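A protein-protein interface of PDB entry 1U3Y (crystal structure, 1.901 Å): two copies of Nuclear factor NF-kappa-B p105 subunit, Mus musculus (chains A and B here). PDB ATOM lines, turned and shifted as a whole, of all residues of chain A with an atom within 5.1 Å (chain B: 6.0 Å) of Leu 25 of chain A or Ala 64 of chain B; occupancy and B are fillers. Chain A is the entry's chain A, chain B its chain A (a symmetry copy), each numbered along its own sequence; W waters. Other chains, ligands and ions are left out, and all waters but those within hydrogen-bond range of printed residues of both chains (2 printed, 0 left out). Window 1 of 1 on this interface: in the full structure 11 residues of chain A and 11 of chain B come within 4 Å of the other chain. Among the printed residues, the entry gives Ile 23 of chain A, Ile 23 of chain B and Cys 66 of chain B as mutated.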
ATOM      1  N   LYS A   5      33.863 -32.795 -25.402  1.00  0.00           N
ATOM      2  CA  LYS A   5      33.255 -33.055 -24.138  1.00  0.00           C
ATOM      3  C   LYS A   5      31.763 -33.225 -24.252  1.00  0.00           C
ATOM      4  O   LYS A   5      31.091 -32.384 -24.845  1.00  0.00           O
ATOM      5  CB  LYS A   5      33.528 -31.921 -23.175  1.00  0.00           C
ATOM      6  CG  LYS A   5      33.213 -32.279 -21.726  1.00  0.00           C
ATOM      7  CD  LYS A   5      33.541 -31.062 -20.836  1.00  0.00           C
ATOM      8  CE  LYS A   5      33.199 -31.305 -19.368  1.00  0.00           C
ATOM      9  NZ  LYS A   5      31.730 -31.352 -19.089  1.00  0.00           N
ATOM     10  N   ILE A   6      31.272 -34.320 -23.684  1.00  0.00           N
ATOM     11  CA  ILE A   6      29.853 -34.529 -23.505  1.00  0.00           C
ATOM     12  C   ILE A   6      29.523 -33.886 -22.158  1.00  0.00           C
ATOM     13  O   ILE A   6      29.989 -34.325 -21.117  1.00  0.00           O
ATOM     14  CB  ILE A   6      29.475 -36.016 -23.521  1.00  0.00           C
ATOM     15  CG1 ILE A   6      29.879 -36.680 -24.836  1.00  0.00           C
ATOM     16  CG2 ILE A   6      27.951 -36.167 -23.271  1.00  0.00           C
ATOM     17  CD1 ILE A   6      29.734 -38.189 -24.867  1.00  0.00           C
ATOM     18  N   VAL A   7      28.764 -32.797 -22.212  1.00  0.00           N
ATOM     19  CA  VAL A   7      28.417 -32.043 -21.032  1.00  0.00           C
ATOM     20  C   VAL A   7      27.176 -32.653 -20.374  1.00  0.00           C
ATOM     21  O   VAL A   7      27.099 -32.780 -19.154  1.00  0.00           O
ATOM     22  CB  VAL A   7      28.208 -30.561 -21.400  1.00  0.00           C
ATOM     23  CG1 VAL A   7      27.635 -29.779 -20.213  1.00  0.00           C
ATOM     24  CG2 VAL A   7      29.515 -29.957 -21.829  1.00  0.00           C
ATOM     25  N   ARG A   8      26.220 -33.094 -21.189  1.00  0.00           N
ATOM     26  CA  ARG A   8      25.022 -33.730 -20.655  1.00  0.00           C
ATOM     27  C   ARG A   8      24.329 -34.559 -21.700  1.00  0.00           C
ATOM     28  O   ARG A   8      24.442 -34.283 -22.861  1.00  0.00           O
ATOM     29  CB  ARG A   8      24.074 -32.662 -20.145  1.00  0.00           C
ATOM     30  CG  ARG A   8      22.988 -33.206 -19.284  1.00  0.00           C
ATOM     31  CD  ARG A   8      22.361 -32.174 -18.393  1.00  0.00           C
ATOM     32  NE  ARG A   8      21.408 -32.826 -17.502  1.00  0.00           N
ATOM     33  CZ  ARG A   8      20.865 -32.261 -16.445  1.00  0.00           C
ATOM     34  NH1 ARG A   8      21.162 -31.001 -16.124  1.00  0.00           N
ATOM     35  NH2 ARG A   8      20.001 -32.958 -15.705  1.00  0.00           N
ATOM     36  N   MET A   9      23.649 -35.607 -21.280  1.00  0.00           N
ATOM     37  CA  MET A   9      22.754 -36.354 -22.160  1.00  0.00           C
ATOM     38  C   MET A   9      21.447 -36.514 -21.435  1.00  0.00           C
ATOM     39  O   MET A   9      21.432 -36.747 -20.239  1.00  0.00           O
ATOM     40  CB  MET A   9      23.319 -37.743 -22.488  1.00  0.00           C
ATOM     41  CG  MET A   9      24.609 -37.732 -23.249  1.00  0.00           C
ATOM     42  SD  MET A   9      25.368 -39.401 -23.402  1.00  0.00           S
ATOM     43  CE  MET A   9      24.294 -40.186 -24.432  1.00  0.00           C
ATOM     44  N   ILE A  23      19.037 -36.159 -26.745  1.00  0.00           N
ATOM     45  CA  ILE A  23      19.704 -34.871 -26.872  1.00  0.00           C
ATOM     46  C   ILE A  23      20.944 -34.852 -26.011  1.00  0.00           C
ATOM     47  O   ILE A  23      20.887 -35.040 -24.792  1.00  0.00           O
ATOM     48  CB  ILE A  23      18.787 -33.668 -26.476  1.00  0.00           C
ATOM     49  CG1 ILE A  23      17.507 -33.664 -27.310  1.00  0.00           C
ATOM     50  CG2 ILE A  23      19.542 -32.365 -26.658  1.00  0.00           C
ATOM     51  CD1 ILE A  23      16.673 -32.411 -27.173  1.00  0.00           C
ATOM     52  N   LEU A  24      22.063 -34.622 -26.680  1.00  0.00           N
ATOM     53  CA  LEU A  24      23.380 -34.526 -26.071  1.00  0.00           C
ATOM     54  C   LEU A  24      23.854 -33.063 -26.162  1.00  0.00           C
ATOM     55  O   LEU A  24      23.744 -32.422 -27.209  1.00  0.00           O
ATOM     56  CB  LEU A  24      24.300 -35.492 -26.826  1.00  0.00           C
ATOM     57  CG  LEU A  24      25.767 -35.605 -26.518  1.00  0.00           C
ATOM     58  CD1 LEU A  24      26.246 -36.986 -26.915  1.00  0.00           C
ATOM     59  CD2 LEU A  24      26.543 -34.476 -27.181  1.00  0.00           C
ATOM     60  N   LEU A  25      24.330 -32.531 -25.040  1.00  0.00           N
ATOM     61  CA  LEU A  25      24.918 -31.200 -24.976  1.00  0.00           C
ATOM     62  C   LEU A  25      26.440 -31.377 -24.955  1.00  0.00           C
ATOM     63  O   LEU A  25      26.962 -32.215 -24.234  1.00  0.00           O
ATOM     64  CB  LEU A  25      24.461 -30.483 -23.712  1.00  0.00           C
ATOM     65  CG  LEU A  25      22.942 -30.291 -23.544  1.00  0.00           C
ATOM     66  CD1 LEU A  25      22.642 -29.469 -22.342  1.00  0.00           C
ATOM     67  CD2 LEU A  25      22.319 -29.700 -24.801  1.00  0.00           C
ATOM     68  N   CYS A  26      27.143 -30.627 -25.773  1.00  0.00           N
ATOM     69  CA  CYS A  26      28.581 -30.850 -25.939  1.00  0.00           C
ATOM     70  C   CYS A  26      29.254 -29.488 -25.941  1.00  0.00           C
ATOM     71  O   CYS A  26      28.621 -28.484 -26.176  1.00  0.00           O
ATOM     72  CB  CYS A  26      28.852 -31.558 -27.285  1.00  0.00           C
ATOM     73  SG  CYS A  26      28.100 -30.886 -28.777  1.00  0.00           S
ATOM     74  N   ASP A  27      30.547 -29.462 -25.723  1.00  0.00           N
ATOM     75  CA  ASP A  27      31.314 -28.263 -26.076  1.00  0.00           C
ATOM     76  C   ASP A  27      31.442 -28.190 -27.570  1.00  0.00           C
ATOM     77  O   ASP A  27      30.955 -29.071 -28.268  1.00  0.00           O
ATOM     78  CB  ASP A  27      32.627 -28.256 -25.326  1.00  0.00           C
ATOM     79  CG  ASP A  27      32.411 -27.894 -23.858  1.00  0.00           C
ATOM     80  OD1 ASP A  27      31.459 -27.099 -23.556  1.00  0.00           O
ATOM     81  OD2 ASP A  27      33.090 -28.376 -22.950  1.00  0.00           O
ATOM     82  N   PHE A  63      26.662 -26.873 -30.474  1.00  0.00           N
ATOM     83  CA  PHE A  63      26.711 -27.088 -29.025  1.00  0.00           C
ATOM     84  C   PHE A  63      25.768 -28.168 -28.502  1.00  0.00           C
ATOM     85  O   PHE A  63      25.720 -28.414 -27.285  1.00  0.00           O
ATOM     86  CB  PHE A  63      26.451 -25.777 -28.313  1.00  0.00           C
ATOM     87  CG  PHE A  63      27.645 -24.850 -28.309  1.00  0.00           C
ATOM     88  CD1 PHE A  63      28.784 -25.188 -27.575  1.00  0.00           C
ATOM     89  CD2 PHE A  63      27.605 -23.640 -28.991  1.00  0.00           C
ATOM     90  CE1 PHE A  63      29.905 -24.348 -27.552  1.00  0.00           C
ATOM     91  CE2 PHE A  63      28.732 -22.784 -28.977  1.00  0.00           C
ATOM     92  CZ  PHE A  63      29.871 -23.149 -28.268  1.00  0.00           C
ATOM     93  N   ALA A  64      24.996 -28.764 -29.405  1.00  0.00           N
ATOM     94  CA  ALA A  64      24.117 -29.885 -29.074  1.00  0.00           C
ATOM     95  C   ALA A  64      23.903 -30.755 -30.282  1.00  0.00           C
ATOM     96  O   ALA A  64      24.035 -30.298 -31.403  1.00  0.00           O
ATOM     97  CB  ALA A  64      22.800 -29.441 -28.503  1.00  0.00           C
ATOM     98  N   ILE A  65      23.576 -32.027 -30.032  1.00  0.00           N
ATOM     99  CA  ILE A  65      23.309 -33.008 -31.067  1.00  0.00           C
ATOM    100  C   ILE A  65      22.068 -33.795 -30.691  1.00  0.00           C
ATOM    101  O   ILE A  65      21.980 -34.381 -29.602  1.00  0.00           O
ATOM    102  CB  ILE A  65      24.485 -33.976 -31.280  1.00  0.00           C
ATOM    103  CG1 ILE A  65      25.790 -33.186 -31.499  1.00  0.00           C
ATOM    104  CG2 ILE A  65      24.154 -34.927 -32.421  1.00  0.00           C
ATOM    105  CD1 ILE A  65      27.014 -34.061 -31.662  1.00  0.00           C
ATOM    106  N   ILE B  23      15.313 -30.928 -21.653  1.00  0.00           N
ATOM    107  CA  ILE B  23      16.300 -30.174 -22.412  1.00  0.00           C
ATOM    108  C   ILE B  23      15.631 -29.489 -23.580  1.00  0.00           C
ATOM    109  O   ILE B  23      15.017 -30.129 -24.439  1.00  0.00           O
ATOM    110  CB  ILE B  23      17.470 -31.066 -22.944  1.00  0.00           C
ATOM    111  CG1 ILE B  23      18.161 -31.798 -21.794  1.00  0.00           C
ATOM    112  CG2 ILE B  23      18.466 -30.208 -23.700  1.00  0.00           C
ATOM    113  CD1 ILE B  23      19.449 -32.490 -22.175  1.00  0.00           C
ATOM    114  N   LEU B  24      15.766 -28.172 -23.583  1.00  0.00           N
ATOM    115  CA  LEU B  24      15.239 -27.294 -24.615  1.00  0.00           C
ATOM    116  C   LEU B  24      16.422 -26.713 -25.412  1.00  0.00           C
ATOM    117  O   LEU B  24      17.416 -26.263 -24.838  1.00  0.00           O
ATOM    118  CB  LEU B  24      14.413 -26.212 -23.910  1.00  0.00           C
ATOM    119  CG  LEU B  24      13.774 -25.078 -24.662  1.00  0.00           C
ATOM    120  CD1 LEU B  24      12.574 -24.586 -23.879  1.00  0.00           C
ATOM    121  CD2 LEU B  24      14.795 -23.990 -24.962  1.00  0.00           C
ATOM    122  N   LEU B  25      16.324 -26.779 -26.736  1.00  0.00           N
ATOM    123  CA  LEU B  25      17.299 -26.181 -27.638  1.00  0.00           C
ATOM    124  C   LEU B  25      16.697 -24.869 -28.153  1.00  0.00           C
ATOM    125  O   LEU B  25      15.535 -24.820 -28.531  1.00  0.00           O
ATOM    126  CB  LEU B  25      17.578 -27.118 -28.806  1.00  0.00           C
ATOM    127  CG  LEU B  25      18.120 -28.515 -28.451  1.00  0.00           C
ATOM    128  CD1 LEU B  25      18.470 -29.275 -29.680  1.00  0.00           C
ATOM    129  CD2 LEU B  25      19.299 -28.421 -27.492  1.00  0.00           C
ATOM    130  N   CYS B  26      17.465 -23.804 -28.123  1.00  0.00           N
ATOM    131  CA  CYS B  26      16.919 -22.482 -28.435  1.00  0.00           C
ATOM    132  C   CYS B  26      17.922 -21.775 -29.331  1.00  0.00           C
ATOM    133  O   CYS B  26      19.076 -22.137 -29.376  1.00  0.00           O
ATOM    134  CB  CYS B  26      16.732 -21.668 -27.134  1.00  0.00           C
ATOM    135  SG  CYS B  26      18.108 -21.571 -25.976  1.00  0.00           S
ATOM    136  N   VAL B  29      20.338 -17.144 -26.443  1.00  0.00           N
ATOM    137  CA  VAL B  29      19.845 -16.378 -25.308  1.00  0.00           C
ATOM    138  C   VAL B  29      20.999 -15.907 -24.402  1.00  0.00           C
ATOM    139  O   VAL B  29      22.127 -16.416 -24.501  1.00  0.00           O
ATOM    140  CB  VAL B  29      18.823 -17.184 -24.435  1.00  0.00           C
ATOM    141  CG1 VAL B  29      17.629 -17.585 -25.255  1.00  0.00           C
ATOM    142  CG2 VAL B  29      19.460 -18.440 -23.797  1.00  0.00           C
ATOM    143  N   ASP B  58      22.513 -23.598 -15.778  1.00  0.00           N
ATOM    144  CA  ASP B  58      21.798 -24.650 -16.534  1.00  0.00           C
ATOM    145  C   ASP B  58      21.578 -24.261 -17.994  1.00  0.00           C
ATOM    146  O   ASP B  58      21.051 -25.049 -18.791  1.00  0.00           O
ATOM    147  CB  ASP B  58      20.432 -24.909 -15.886  1.00  0.00           C
ATOM    148  CG  ASP B  58      20.535 -25.440 -14.473  1.00  0.00           C
ATOM    149  OD1 ASP B  58      21.336 -26.339 -14.262  1.00  0.00           O
ATOM    150  OD2 ASP B  58      19.839 -25.048 -13.515  1.00  0.00           O
ATOM    151  N   VAL B  59      21.963 -23.038 -18.343  1.00  0.00           N
ATOM    152  CA  VAL B  59      21.963 -22.589 -19.726  1.00  0.00           C
ATOM    153  C   VAL B  59      23.293 -22.954 -20.341  1.00  0.00           C
ATOM    154  O   VAL B  59      24.354 -22.528 -19.853  1.00  0.00           O
ATOM    155  CB  VAL B  59      21.660 -21.074 -19.813  1.00  0.00           C
ATOM    156  CG1 VAL B  59      21.628 -20.587 -21.254  1.00  0.00           C
ATOM    157  CG2 VAL B  59      20.361 -20.719 -19.031  1.00  0.00           C
ATOM    158  N   HIS B  60      23.232 -23.759 -21.408  1.00  0.00           N
ATOM    159  CA  HIS B  60      24.401 -24.348 -21.997  1.00  0.00           C
ATOM    160  C   HIS B  60      24.833 -23.515 -23.192  1.00  0.00           C
ATOM    161  O   HIS B  60      24.230 -23.567 -24.278  1.00  0.00           O
ATOM    162  CB  HIS B  60      24.156 -25.824 -22.396  1.00  0.00           C
ATOM    163  CG  HIS B  60      25.262 -26.402 -23.208  1.00  0.00           C
ATOM    164  ND1 HIS B  60      26.550 -26.526 -22.719  1.00  0.00           N
ATOM    165  CD2 HIS B  60      25.285 -26.894 -24.471  1.00  0.00           C
ATOM    166  CE1 HIS B  60      27.324 -27.029 -23.671  1.00  0.00           C
ATOM    167  NE2 HIS B  60      26.573 -27.290 -24.730  1.00  0.00           N
ATOM    168  N   ARG B  61      25.876 -22.735 -22.979  1.00  0.00           N
ATOM    169  CA  ARG B  61      26.552 -21.973 -24.029  1.00  0.00           C
ATOM    170  C   ARG B  61      25.572 -21.132 -24.861  1.00  0.00           C
ATOM    171  O   ARG B  61      25.742 -21.002 -26.057  1.00  0.00           O
ATOM    172  CB  ARG B  61      27.397 -22.900 -24.921  1.00  0.00           C
ATOM    173  CG  ARG B  61      28.542 -23.638 -24.186  1.00  0.00           C
ATOM    174  CD  ARG B  61      29.488 -22.745 -23.399  1.00  0.00           C
ATOM    175  NE  ARG B  61      29.731 -21.462 -24.080  1.00  0.00           N
ATOM    176  CZ  ARG B  61      30.745 -21.213 -24.909  1.00  0.00           C
ATOM    177  NH1 ARG B  61      31.665 -22.135 -25.153  1.00  0.00           N
ATOM    178  NH2 ARG B  61      30.843 -20.023 -25.492  1.00  0.00           N
ATOM    179  N   GLN B  62      24.538 -20.625 -24.187  1.00  0.00           N
ATOM    180  CA  GLN B  62      23.540 -19.724 -24.773  1.00  0.00           C
ATOM    181  C   GLN B  62      22.604 -20.385 -25.802  1.00  0.00           C
ATOM    182  O   GLN B  62      21.765 -19.712 -26.412  1.00  0.00           O
ATOM    183  CB  GLN B  62      24.266 -18.514 -25.406  1.00  0.00           C
ATOM    184  CG  GLN B  62      25.029 -17.731 -24.400  1.00  0.00           C
ATOM    185  CD  GLN B  62      25.673 -16.500 -25.002  1.00  0.00           C
ATOM    186  OE1 GLN B  62      25.180 -15.391 -24.822  1.00  0.00           O
ATOM    187  NE2 GLN B  62      26.730 -16.703 -25.777  1.00  0.00           N
ATOM    188  N   PHE B  63      22.695 -21.699 -25.968  1.00  0.00           N
ATOM    189  CA  PHE B  63      21.939 -22.357 -27.037  1.00  0.00           C
ATOM    190  C   PHE B  63      21.063 -23.521 -26.586  1.00  0.00           C
ATOM    191  O   PHE B  63      20.396 -24.157 -27.420  1.00  0.00           O
ATOM    192  CB  PHE B  63      22.894 -22.811 -28.122  1.00  0.00           C
ATOM    193  CG  PHE B  63      23.362 -21.686 -29.017  1.00  0.00           C
ATOM    194  CD1 PHE B  63      22.457 -21.059 -29.876  1.00  0.00           C
ATOM    195  CD2 PHE B  63      24.697 -21.299 -29.028  1.00  0.00           C
ATOM    196  CE1 PHE B  63      22.863 -20.016 -30.718  1.00  0.00           C
ATOM    197  CE2 PHE B  63      25.118 -20.244 -29.873  1.00  0.00           C
ATOM    198  CZ  PHE B  63      24.199 -19.608 -30.699  1.00  0.00           C
ATOM    199  N   ALA B  64      21.106 -23.824 -25.291  1.00  0.00           N
ATOM    200  CA  ALA B  64      20.248 -24.845 -24.692  1.00  0.00           C
ATOM    201  C   ALA B  64      20.007 -24.538 -23.240  1.00  0.00           C
ATOM    202  O   ALA B  64      20.798 -23.856 -22.614  1.00  0.00           O
ATOM    203  CB  ALA B  64      20.800 -26.234 -24.853  1.00  0.00           C
ATOM    204  N   ILE B  65      18.889 -25.048 -22.715  1.00  0.00           N
ATOM    205  CA  ILE B  65      18.499 -24.878 -21.328  1.00  0.00           C
ATOM    206  C   ILE B  65      18.022 -26.211 -20.783  1.00  0.00           C
ATOM    207  O   ILE B  65      17.117 -26.850 -21.340  1.00  0.00           O
ATOM    208  CB  ILE B  65      17.391 -23.826 -21.151  1.00  0.00           C
ATOM    209  CG1 ILE B  65      17.792 -22.510 -21.847  1.00  0.00           C
ATOM    210  CG2 ILE B  65      17.087 -23.659 -19.670  1.00  0.00           C
ATOM    211  CD1 ILE B  65      16.733 -21.432 -21.772  1.00  0.00           C
ATOM    212  N   CYS B  66      18.649 -26.632 -19.691  1.00  0.00           N
ATOM    213  CA  CYS B  66      18.157 -27.768 -18.910  1.00  0.00           C
ATOM    214  C   CYS B  66      17.354 -27.239 -17.740  1.00  0.00           C
ATOM    215  O   CYS B  66      17.866 -26.430 -16.957  1.00  0.00           O
ATOM    216  CB  CYS B  66      19.326 -28.573 -18.346  1.00  0.00           C
ATOM    217  SG  CYS B  66      20.414 -29.228 -19.605  1.00  0.00           S
HETATM  218  O   HOH W   1      31.966 -24.632 -24.045  1.00  0.00           O
HETATM  219  O   HOH W   2      22.195 -28.456 -16.442  1.00  0.00           O
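Ile 23 of chain A touches its own counterpart, Ile 23 of chain B.
Leu 25 of chain A touches Ala 64 of chain B, and with the chains exchanged Ala 64 of chain A touches Leu 25 of chain B.
Phe 63 of chain A touches its own counterpart, Phe 63 of chain B.
Positions printed for both chains: 23, 24, 25, 26, 63, 64 and 65.
Of the 10 pairs that touch across the chains among the printed residues, 4 have their exchanged pair printed and touching as well.
The backbone NH (N) of Val 7 of chain A sits at hydrogen-bond distance from the backbone carbonyl oxygen (O) of Leu 25 of chain A (2.8 Å).
The backbone carbonyl oxygen (O) of Arg 8 of chain A is in hydrogen-bond range of the backbone NH (N) of Leu 25 of chain A (2.8 Å).
The backbone NH (N) of Cys 26 of chain A lies within hydrogen-bond range of the backbone carbonyl oxygen (O) of Phe 63 of chain A.
O of Phe 63 of chain B lies within hydrogen-bond range of N of Cys 26 of chain B (3.0 Å).
The backbone NH of Cys 66 of chain B is in hydrogen-bond range of the backbone carbonyl oxygen of Asp 58 of chain B (3.0 Å).
Among the printed residues, merely in contact across the chains: Arg 8 of chain A with Cys 66 of chain B, Ile 23 of chain A with Ile 23 of chain B, Leu 25 of chain A with His 60 of chain B, Leu 25 of chain A with Ala 64 of chain B, Leu 25 of chain A with Cys 66 of chain B, Phe 63 of chain A with Arg 61 of chain B, Phe 63 of chain A with Phe 63 of chain B and Ala 64 of chain A with Leu 25 of chain B.
Leu 25 of chain A touches just these residues of chain B: His 60 (3.8 Å), Ala 64 (3.8 Å) and Cys 66 (3.5 Å).
Ala 64 of chain B touches just one residue of chain A: Leu 25 (3.8 Å).
Printed residues of chain B within 4 Å of Arg 8 of chain A: Cys 66.
Printed residues of chain A within 4 Å of Leu 25 of chain B: Ala 64 (3.8 Å).
Of the printed residues of chain B, Ile 23 of chain A touches Ile 23.
Of the printed residues of chain B, Ala 64 of chain A touches Leu 25 (3.8 Å).
Of the printed residues of chain A, Cys 66 of chain B touches Arg 8 (3.7 Å) and Leu 25 (3.5 Å).
Asp 58 of chain B touches none of the printed residues of chain A.
Gln 62 of chain B touches none of the printed residues of chain A.
The nearest printed residue of chain A that does not touch Leu 25 of chain B is Ile 23 of chain A (4.04 Å).
O of Cys 26 of chain A is in hydrogen-bond range of NE2 of His 60 of chain B, 2.8 Å away.
O of Phe 63 of chain A lies within hydrogen-bond range of NE2 of His 60 of chain B (2.9 Å).
Printed residues of chain B that touch a printed residue of chain A: Ile 23, Leu 25, His 60, Arg 61, Phe 63, Ala 64 and Cys 66.
Among the printed residues, 10 pairs touch across the chains.
Water W1 lies within hydrogen-bond range of the side-chain carboxylate (OD1) of Asp 27 of chain A and the guanidinium group (NH1) of Arg 61 of chain B.
Water W2 lies within hydrogen-bond range of NH1 of Arg 8 of chain A (2.8 Å), OD1 of Asp 58 of chain B (3.2 Å) and SG of Cys 66 of chain B (3.7 Å).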
